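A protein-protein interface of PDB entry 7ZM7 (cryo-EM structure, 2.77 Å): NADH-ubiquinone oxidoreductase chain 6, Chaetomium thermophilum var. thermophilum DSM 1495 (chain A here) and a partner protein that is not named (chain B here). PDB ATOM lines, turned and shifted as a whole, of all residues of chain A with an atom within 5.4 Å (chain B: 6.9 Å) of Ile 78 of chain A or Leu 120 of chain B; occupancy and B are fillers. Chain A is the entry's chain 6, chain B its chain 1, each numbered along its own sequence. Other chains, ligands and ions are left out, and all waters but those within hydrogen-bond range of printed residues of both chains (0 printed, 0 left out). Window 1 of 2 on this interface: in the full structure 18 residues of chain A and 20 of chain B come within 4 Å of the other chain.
The backbone carbonyl oxygen of Ile 78 of chain A lies within hydrogen-bond range of the side-chain hydroxyl of Tyr 123 of chain B. The side-chain hydroxyl (OH) of Tyr 123 of chain B lies close to the side-chain hydroxyl (OG) of Ser 82 of chain A (2.3 Å).
The side-chain hydroxyl (OG) of Ser 82 of chain A sits at hydrogen-bond distance from the backbone carbonyl oxygen (O) of Ile 78 of chain A (3.0 Å). The backbone NH (N) of Gly 79 of chain A is in hydrogen-bond range of the backbone carbonyl oxygen (O) of Leu 74 of chain A (3.0 Å). O of Ser 119 of chain B sits at hydrogen-bond distance from OG1 of Thr 122 of chain B, at 2.9 Å. The backbone carbonyl oxygen (O) of Ala 116 of chain B lies within hydrogen-bond range of the side-chain hydroxyl (OG) of Ser 119 of chain B, at 2.7 Å. N of Ser 82 of chain A is in hydrogen-bond range of O of Tyr 77 of chain A (2.9 Å). The side-chain hydroxyl of Ser 119 of chain B is in hydrogen-bond range of the backbone carbonyl oxygen of Leu 115 of chain B (3.4 Å).
CD1 of Ile 51 of chain A touches CE1 of Tyr 123 of chain B (3.7 Å). CB of Ala 116 of chain B touches CD1 of Leu 74 of chain A, 3.9 Å away. Leu 115 of chain B touches Ile 75 of chain A (CB to CD1, 3.6 Å). Ile 75 of chain A touches Ala 116 of chain B (CG1 to CA, 3.9 Å). Ile 78 of chain A touches Leu 120 of chain B. CA of Gly 79 of chain A touches CB of Ser 119 of chain B, 3.8 Å away. Ile 83 of chain A touches Thr 122 of chain B (CD1 to OG1, 3.7 Å). Ile 83 of chain A touches Tyr 123 of chain B (CD1 to CZ, 3.8 Å).
Ala 55 of chain A touches none of the printed residues of chain B. Printed residues of chain B within 4 Å of Leu 74 of chain A: Ala 116 (3.9 Å). Tyr 77 of chain A touches none of the printed residues of chain B. Of chain B, only Leu 120 and Tyr 123 come within 4 Å of Ile 78 of chain A. Of the printed residues of chain B, Ser 82 of chain A touches Tyr 123 (2.3 Å). Of chain A, only Ile 78 (3.7 Å) comes within 4 Å of Leu 120 of chain B. Printed residues of chain A within 4 Å of Thr 122 of chain B: Ile 83. Printed residues of chain A within 4 Å of Tyr 123 of chain B: Ile 51, Ile 78, Ser 82 and Ile 83. The nearest residue of chain B that does not touch Ile 78 of chain A is Ser 119 of chain B (4.8 Å). The nearest printed residue of chain A that does not touch Leu 120 of chain B is Leu 74 of chain A (5.5 Å). The nearest printed residue of chain A that does not touch Leu 115 of chain B is Leu 74 of chain A (6.5 Å).
Hydrophobic or aromatic side chains of chain B that line the printed part of chain A: Leu 115, Ala 116, Leu 120 and Tyr 123. Of the 14 printed residues of chain A, 7 touch a printed residue of chain B. Hydrophobic or aromatic side chains of chain A within 4 Å of the printed part of chain B: Ile 51, Leu 74, Ile 75, Ile 78 and Ile 83. Among the printed residues, 10 pairs touch across the chains. Among the printed residues, no Asp or Glu carboxylate lies within 4 Å of a Lys or Arg side-chain nitrogen of the other chain.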
ATOM      1  N   ILE A  51       0.277  30.812 -11.065  1.00  0.00           N
ATOM      2  CA  ILE A  51       1.590  30.322 -11.462  1.00  0.00           C
ATOM      3  C   ILE A  51       1.703  30.321 -12.976  1.00  0.00           C
ATOM      4  O   ILE A  51       2.781  30.556 -13.531  1.00  0.00           O
ATOM      5  CB  ILE A  51       1.864  28.929 -10.864  1.00  0.00           C
ATOM      6  CG1 ILE A  51       1.705  28.955  -9.355  1.00  0.00           C
ATOM      7  CG2 ILE A  51       3.269  28.485 -11.166  1.00  0.00           C
ATOM      8  CD1 ILE A  51       1.386  27.628  -8.768  1.00  0.00           C
ATOM      9  N   PHE A  54       2.248  34.109 -14.131  1.00  0.00           N
ATOM     10  CA  PHE A  54       3.608  34.565 -13.878  1.00  0.00           C
ATOM     11  C   PHE A  54       4.581  33.985 -14.890  1.00  0.00           C
ATOM     12  O   PHE A  54       5.556  34.644 -15.263  1.00  0.00           O
ATOM     13  CB  PHE A  54       4.037  34.199 -12.457  1.00  0.00           C
ATOM     14  CG  PHE A  54       3.429  35.072 -11.413  1.00  0.00           C
ATOM     15  CD1 PHE A  54       3.432  36.440 -11.558  1.00  0.00           C
ATOM     16  CD2 PHE A  54       2.826  34.530 -10.300  1.00  0.00           C
ATOM     17  CE1 PHE A  54       2.858  37.248 -10.613  1.00  0.00           C
ATOM     18  CE2 PHE A  54       2.259  35.340  -9.355  1.00  0.00           C
ATOM     19  CZ  PHE A  54       2.274  36.706  -9.518  1.00  0.00           C
ATOM     20  N   ALA A  55       4.339  32.753 -15.337  1.00  0.00           N
ATOM     21  CA  ALA A  55       5.190  32.149 -16.353  1.00  0.00           C
ATOM     22  C   ALA A  55       5.048  32.849 -17.696  1.00  0.00           C
ATOM     23  O   ALA A  55       6.049  33.112 -18.365  1.00  0.00           O
ATOM     24  CB  ALA A  55       4.869  30.664 -16.493  1.00  0.00           C
ATOM     25  N   TYR A  73      11.746  36.966 -11.965  1.00  0.00           N
ATOM     26  CA  TYR A  73      10.336  36.680 -11.734  1.00  0.00           C
ATOM     27  C   TYR A  73      10.111  35.197 -11.562  1.00  0.00           C
ATOM     28  O   TYR A  73       9.321  34.772 -10.716  1.00  0.00           O
ATOM     29  CB  TYR A  73       9.490  37.174 -12.902  1.00  0.00           C
ATOM     30  CG  TYR A  73       9.094  38.616 -12.875  1.00  0.00           C
ATOM     31  CD1 TYR A  73       8.062  39.058 -12.065  1.00  0.00           C
ATOM     32  CD2 TYR A  73       9.709  39.520 -13.701  1.00  0.00           C
ATOM     33  CE1 TYR A  73       7.684  40.361 -12.061  1.00  0.00           C
ATOM     34  CE2 TYR A  73       9.345  40.825 -13.709  1.00  0.00           C
ATOM     35  CZ  TYR A  73       8.334  41.245 -12.893  1.00  0.00           C
ATOM     36  OH  TYR A  73       7.999  42.568 -12.922  1.00  0.00           O
ATOM     37  N   LEU A  74      10.769  34.394 -12.392  1.00  0.00           N
ATOM     38  CA  LEU A  74      10.655  32.950 -12.281  1.00  0.00           C
ATOM     39  C   LEU A  74      11.158  32.469 -10.930  1.00  0.00           C
ATOM     40  O   LEU A  74      10.461  31.734 -10.222  1.00  0.00           O
ATOM     41  CB  LEU A  74      11.431  32.291 -13.417  1.00  0.00           C
ATOM     42  CG  LEU A  74      10.682  32.101 -14.720  1.00  0.00           C
ATOM     43  CD1 LEU A  74      11.457  31.166 -15.618  1.00  0.00           C
ATOM     44  CD2 LEU A  74       9.295  31.555 -14.457  1.00  0.00           C
ATOM     45  N   ILE A  75      12.346  32.915 -10.532  1.00  0.00           N
ATOM     46  CA  ILE A  75      12.945  32.474  -9.278  1.00  0.00           C
ATOM     47  C   ILE A  75      12.135  32.958  -8.081  1.00  0.00           C
ATOM     48  O   ILE A  75      12.060  32.279  -7.055  1.00  0.00           O
ATOM     49  CB  ILE A  75      14.408  32.945  -9.205  1.00  0.00           C
ATOM     50  CG1 ILE A  75      15.270  32.162 -10.184  1.00  0.00           C
ATOM     51  CG2 ILE A  75      14.968  32.802  -7.824  1.00  0.00           C
ATOM     52  CD1 ILE A  75      16.687  32.575 -10.167  1.00  0.00           C
ATOM     53  N   VAL A  76      11.531  34.133  -8.175  1.00  0.00           N
ATOM     54  CA  VAL A  76      10.937  34.762  -7.003  1.00  0.00           C
ATOM     55  C   VAL A  76       9.464  34.411  -6.856  1.00  0.00           C
ATOM     56  O   VAL A  76       9.024  34.017  -5.776  1.00  0.00           O
ATOM     57  CB  VAL A  76      11.162  36.288  -7.052  1.00  0.00           C
ATOM     58  CG1 VAL A  76      10.168  36.999  -6.178  1.00  0.00           C
ATOM     59  CG2 VAL A  76      12.580  36.627  -6.616  1.00  0.00           C
ATOM     60  N   TYR A  77       8.679  34.569  -7.922  1.00  0.00           N
ATOM     61  CA  TYR A  77       7.214  34.345  -7.798  1.00  0.00           C
ATOM     62  C   TYR A  77       6.875  32.865  -7.854  1.00  0.00           C
ATOM     63  O   TYR A  77       6.372  32.325  -6.860  1.00  0.00           O
ATOM     64  CB  TYR A  77       6.434  35.169  -8.820  1.00  0.00           C
ATOM     65  CG  TYR A  77       6.411  36.606  -8.388  1.00  0.00           C
ATOM     66  CD1 TYR A  77       5.658  36.989  -7.294  1.00  0.00           C
ATOM     67  CD2 TYR A  77       7.226  37.543  -8.991  1.00  0.00           C
ATOM     68  CE1 TYR A  77       5.665  38.294  -6.842  1.00  0.00           C
ATOM     69  CE2 TYR A  77       7.241  38.854  -8.557  1.00  0.00           C
ATOM     70  CZ  TYR A  77       6.461  39.224  -7.480  1.00  0.00           C
ATOM     71  OH  TYR A  77       6.479  40.508  -7.041  1.00  0.00           O
ATOM     72  N   ILE A  78       7.141  32.247  -8.997  1.00  0.00           N
ATOM     73  CA  ILE A  78       6.852  30.829  -9.127  1.00  0.00           C
ATOM     74  C   ILE A  78       7.724  30.033  -8.180  1.00  0.00           C
ATOM     75  O   ILE A  78       7.298  29.018  -7.628  1.00  0.00           O
ATOM     76  CB  ILE A  78       7.040  30.384 -10.583  1.00  0.00           C
ATOM     77  CG1 ILE A  78       6.067  31.118 -11.491  1.00  0.00           C
ATOM     78  CG2 ILE A  78       6.885  28.880 -10.721  1.00  0.00           C
ATOM     79  CD1 ILE A  78       6.122  30.647 -12.886  1.00  0.00           C
ATOM     80  N   GLY A  79       8.954  30.486  -7.964  1.00  0.00           N
ATOM     81  CA  GLY A  79       9.860  29.743  -7.117  1.00  0.00           C
ATOM     82  C   GLY A  79       9.438  29.721  -5.662  1.00  0.00           C
ATOM     83  O   GLY A  79       9.485  28.674  -5.013  1.00  0.00           O
ATOM     84  N   ALA A  80       9.038  30.868  -5.127  1.00  0.00           N
ATOM     85  CA  ALA A  80       8.989  31.028  -3.680  1.00  0.00           C
ATOM     86  C   ALA A  80       7.697  31.618  -3.145  1.00  0.00           C
ATOM     87  O   ALA A  80       7.252  31.210  -2.079  1.00  0.00           O
ATOM     88  CB  ALA A  80      10.162  31.897  -3.224  1.00  0.00           C
ATOM     89  N   VAL A  81       7.092  32.586  -3.833  1.00  0.00           N
ATOM     90  CA  VAL A  81       5.872  33.201  -3.321  1.00  0.00           C
ATOM     91  C   VAL A  81       4.696  32.249  -3.472  1.00  0.00           C
ATOM     92  O   VAL A  81       3.925  32.028  -2.535  1.00  0.00           O
ATOM     93  CB  VAL A  81       5.586  34.542  -4.028  1.00  0.00           C
ATOM     94  CG1 VAL A  81       4.296  35.160  -3.488  1.00  0.00           C
ATOM     95  CG2 VAL A  81       6.719  35.513  -3.872  1.00  0.00           C
ATOM     96  N   SER A  82       4.530  31.690  -4.664  1.00  0.00           N
ATOM     97  CA  SER A  82       3.425  30.775  -4.904  1.00  0.00           C
ATOM     98  C   SER A  82       3.589  29.477  -4.129  1.00  0.00           C
ATOM     99  O   SER A  82       2.604  28.772  -3.898  1.00  0.00           O
ATOM    100  CB  SER A  82       3.306  30.502  -6.399  1.00  0.00           C
ATOM    101  OG  SER A  82       4.486  29.910  -6.894  1.00  0.00           O
ATOM    102  N   ILE A  83       4.818  29.137  -3.744  1.00  0.00           N
ATOM    103  CA  ILE A  83       5.043  27.973  -2.895  1.00  0.00           C
ATOM    104  C   ILE A  83       4.529  28.236  -1.491  1.00  0.00           C
ATOM    105  O   ILE A  83       3.862  27.390  -0.893  1.00  0.00           O
ATOM    106  CB  ILE A  83       6.531  27.592  -2.897  1.00  0.00           C
ATOM    107  CG1 ILE A  83       6.881  26.816  -4.165  1.00  0.00           C
ATOM    108  CG2 ILE A  83       6.871  26.781  -1.682  1.00  0.00           C
ATOM    109  CD1 ILE A  83       6.131  25.533  -4.345  1.00  0.00           C
ATOM    110  N   THR B  85       6.892  17.633 -15.660  1.00  0.00           N
ATOM    111  CA  THR B  85       7.914  17.480 -14.603  1.00  0.00           C
ATOM    112  C   THR B  85       9.136  16.935 -15.334  1.00  0.00           C
ATOM    113  O   THR B  85      10.266  17.313 -14.965  1.00  0.00           O
ATOM    114  CB  THR B  85       7.454  16.480 -13.544  1.00  0.00           C
ATOM    115  OG1 THR B  85       6.210  16.948 -13.022  1.00  0.00           O
ATOM    116  CG2 THR B  85       8.449  16.314 -12.416  1.00  0.00           C
ATOM    117  N   PHE B  88      10.804  19.715 -17.179  1.00  0.00           N
ATOM    118  CA  PHE B  88      11.556  20.633 -16.282  1.00  0.00           C
ATOM    119  C   PHE B  88      12.828  19.916 -15.837  1.00  0.00           C
ATOM    120  O   PHE B  88      13.714  20.548 -15.236  1.00  0.00           O
ATOM    121  CB  PHE B  88      10.703  21.046 -15.082  1.00  0.00           C
ATOM    122  CG  PHE B  88       9.591  22.012 -15.399  1.00  0.00           C
ATOM    123  CD1 PHE B  88       9.612  22.758 -16.566  1.00  0.00           C
ATOM    124  CD2 PHE B  88       8.531  22.184 -14.525  1.00  0.00           C
ATOM    125  CE1 PHE B  88       8.591  23.648 -16.858  1.00  0.00           C
ATOM    126  CE2 PHE B  88       7.512  23.077 -14.815  1.00  0.00           C
ATOM    127  CZ  PHE B  88       7.544  23.806 -15.981  1.00  0.00           C
ATOM    128  N   LEU B  91      15.155  20.365 -19.281  1.00  0.00           N
ATOM    129  CA  LEU B  91      15.351  21.760 -19.778  1.00  0.00           C
ATOM    130  C   LEU B  91      16.672  22.351 -19.285  1.00  0.00           C
ATOM    131  O   LEU B  91      17.070  23.398 -19.815  1.00  0.00           O
ATOM    132  CB  LEU B  91      14.184  22.644 -19.324  1.00  0.00           C
ATOM    133  CG  LEU B  91      13.076  22.857 -20.350  1.00  0.00           C
ATOM    134  CD1 LEU B  91      12.053  23.854 -19.835  1.00  0.00           C
ATOM    135  CD2 LEU B  91      13.654  23.325 -21.676  1.00  0.00           C
ATOM    136  N   LEU B 115      18.888  28.182 -12.267  1.00  0.00           N
ATOM    137  CA  LEU B 115      18.382  28.487 -10.910  1.00  0.00           C
ATOM    138  C   LEU B 115      16.875  28.611 -11.065  1.00  0.00           C
ATOM    139  O   LEU B 115      16.156  28.318 -10.100  1.00  0.00           O
ATOM    140  CB  LEU B 115      19.015  29.786 -10.407  1.00  0.00           C
ATOM    141  CG  LEU B 115      20.408  29.646  -9.796  1.00  0.00           C
ATOM    142  CD1 LEU B 115      20.901  30.985  -9.275  1.00  0.00           C
ATOM    143  CD2 LEU B 115      20.408  28.613  -8.682  1.00  0.00           C
ATOM    144  N   ALA B 116      16.434  29.031 -12.258  1.00  0.00           N
ATOM    145  CA  ALA B 116      14.999  29.088 -12.522  1.00  0.00           C
ATOM    146  C   ALA B 116      14.404  27.699 -12.691  1.00  0.00           C
ATOM    147  O   ALA B 116      13.356  27.400 -12.114  1.00  0.00           O
ATOM    148  CB  ALA B 116      14.712  29.934 -13.757  1.00  0.00           C
ATOM    149  N   VAL B 117      15.055  26.877 -13.515  1.00  0.00           N
ATOM    150  CA  VAL B 117      14.552  25.499 -13.800  1.00  0.00           C
ATOM    151  C   VAL B 117      14.593  24.659 -12.522  1.00  0.00           C
ATOM    152  O   VAL B 117      13.886  23.637 -12.475  1.00  0.00           O
ATOM    153  CB  VAL B 117      15.285  24.823 -14.974  1.00  0.00           C
ATOM    154  CG1 VAL B 117      15.115  25.591 -16.275  1.00  0.00           C
ATOM    155  CG2 VAL B 117      16.753  24.564 -14.679  1.00  0.00           C
ATOM    156  N   SER B 118      15.380  25.074 -11.530  1.00  0.00           N
ATOM    157  CA  SER B 118      15.535  24.249 -10.308  1.00  0.00           C
ATOM    158  C   SER B 118      14.404  24.574  -9.345  1.00  0.00           C
ATOM    159  O   SER B 118      13.954  23.669  -8.638  1.00  0.00           O
ATOM    160  CB  SER B 118      16.858  24.512  -9.662  1.00  0.00           C
ATOM    161  OG  SER B 118      17.027  23.692  -8.516  1.00  0.00           O
ATOM    162  N   SER B 119      13.979  25.832  -9.319  1.00  0.00           N
ATOM    163  CA  SER B 119      12.871  26.207  -8.458  1.00  0.00           C
ATOM    164  C   SER B 119      11.555  25.622  -8.944  1.00  0.00           C
ATOM    165  O   SER B 119      10.570  25.616  -8.202  1.00  0.00           O
ATOM    166  CB  SER B 119      12.802  27.728  -8.363  1.00  0.00           C
ATOM    167  OG  SER B 119      12.812  28.322  -9.643  1.00  0.00           O
ATOM    168  N   LEU B 120      11.515  25.138 -10.181  1.00  0.00           N
ATOM    169  CA  LEU B 120      10.354  24.411 -10.666  1.00  0.00           C
ATOM    170  C   LEU B 120      10.347  22.962 -10.207  1.00  0.00           C
ATOM    171  O   LEU B 120       9.328  22.284 -10.353  1.00  0.00           O
ATOM    172  CB  LEU B 120      10.306  24.468 -12.185  1.00  0.00           C
ATOM    173  CG  LEU B 120      10.148  25.846 -12.827  1.00  0.00           C
ATOM    174  CD1 LEU B 120      10.514  25.788 -14.283  1.00  0.00           C
ATOM    175  CD2 LEU B 120       8.751  26.370 -12.674  1.00  0.00           C
ATOM    176  N   ALA B 121      11.457  22.474  -9.659  1.00  0.00           N
ATOM    177  CA  ALA B 121      11.498  21.078  -9.176  1.00  0.00           C
ATOM    178  C   ALA B 121      10.517  20.938  -8.018  1.00  0.00           C
ATOM    179  O   ALA B 121       9.898  19.870  -7.904  1.00  0.00           O
ATOM    180  CB  ALA B 121      12.895  20.727  -8.726  1.00  0.00           C
ATOM    181  N   THR B 122      10.402  21.966  -7.179  1.00  0.00           N
ATOM    182  CA  THR B 122       9.539  21.877  -6.012  1.00  0.00           C
ATOM    183  C   THR B 122       8.103  21.546  -6.374  1.00  0.00           C
ATOM    184  O   THR B 122       7.377  20.998  -5.545  1.00  0.00           O
ATOM    185  CB  THR B 122       9.571  23.190  -5.243  1.00  0.00           C
ATOM    186  OG1 THR B 122       9.152  24.247  -6.112  1.00  0.00           O
ATOM    187  CG2 THR B 122      10.949  23.472  -4.724  1.00  0.00           C
ATOM    188  N   TYR B 123       7.674  21.867  -7.588  1.00  0.00           N
ATOM    189  CA  TYR B 123       6.301  21.595  -7.985  1.00  0.00           C
ATOM    190  C   TYR B 123       6.083  20.128  -8.297  1.00  0.00           C
ATOM    191  O   TYR B 123       4.991  19.612  -8.076  1.00  0.00           O
ATOM    192  CB  TYR B 123       5.925  22.478  -9.175  1.00  0.00           C
ATOM    193  CG  TYR B 123       5.703  23.898  -8.763  1.00  0.00           C
ATOM    194  CD1 TYR B 123       4.522  24.275  -8.155  1.00  0.00           C
ATOM    195  CD2 TYR B 123       6.679  24.860  -8.950  1.00  0.00           C
ATOM    196  CE1 TYR B 123       4.307  25.580  -7.752  1.00  0.00           C
ATOM    197  CE2 TYR B 123       6.478  26.170  -8.542  1.00  0.00           C
ATOM    198  CZ  TYR B 123       5.290  26.520  -7.950  1.00  0.00           C
ATOM    199  OH  TYR B 123       5.069  27.805  -7.546  1.00  0.00           O
ATOM    200  N   GLY B 124       7.136  19.440  -8.737  1.00  0.00           N
ATOM    201  CA  GLY B 124       6.994  18.029  -9.143  1.00  0.00           C
ATOM    202  C   GLY B 124       7.061  17.103  -7.949  1.00  0.00           C
ATOM    203  O   GLY B 124       6.794  15.906  -8.121  1.00  0.00           O
ATOM    204  N   ILE B 125       7.338  17.655  -6.769  1.00  0.00           N
ATOM    205  CA  ILE B 125       7.378  16.831  -5.526  1.00  0.00           C
ATOM    206  C   ILE B 125       6.154  17.241  -4.718  1.00  0.00           C
ATOM    207  O   ILE B 125       5.556  16.373  -4.057  1.00  0.00           O
ATOM    208  CB  ILE B 125       8.708  17.036  -4.771  1.00  0.00           C
ATOM    209  CG1 ILE B 125       9.827  16.200  -5.393  1.00  0.00           C
ATOM    210  CG2 ILE B 125       8.558  16.738  -3.289  1.00  0.00           C
ATOM    211  CD1 ILE B 125       9.479  14.741  -5.499  1.00  0.00           C
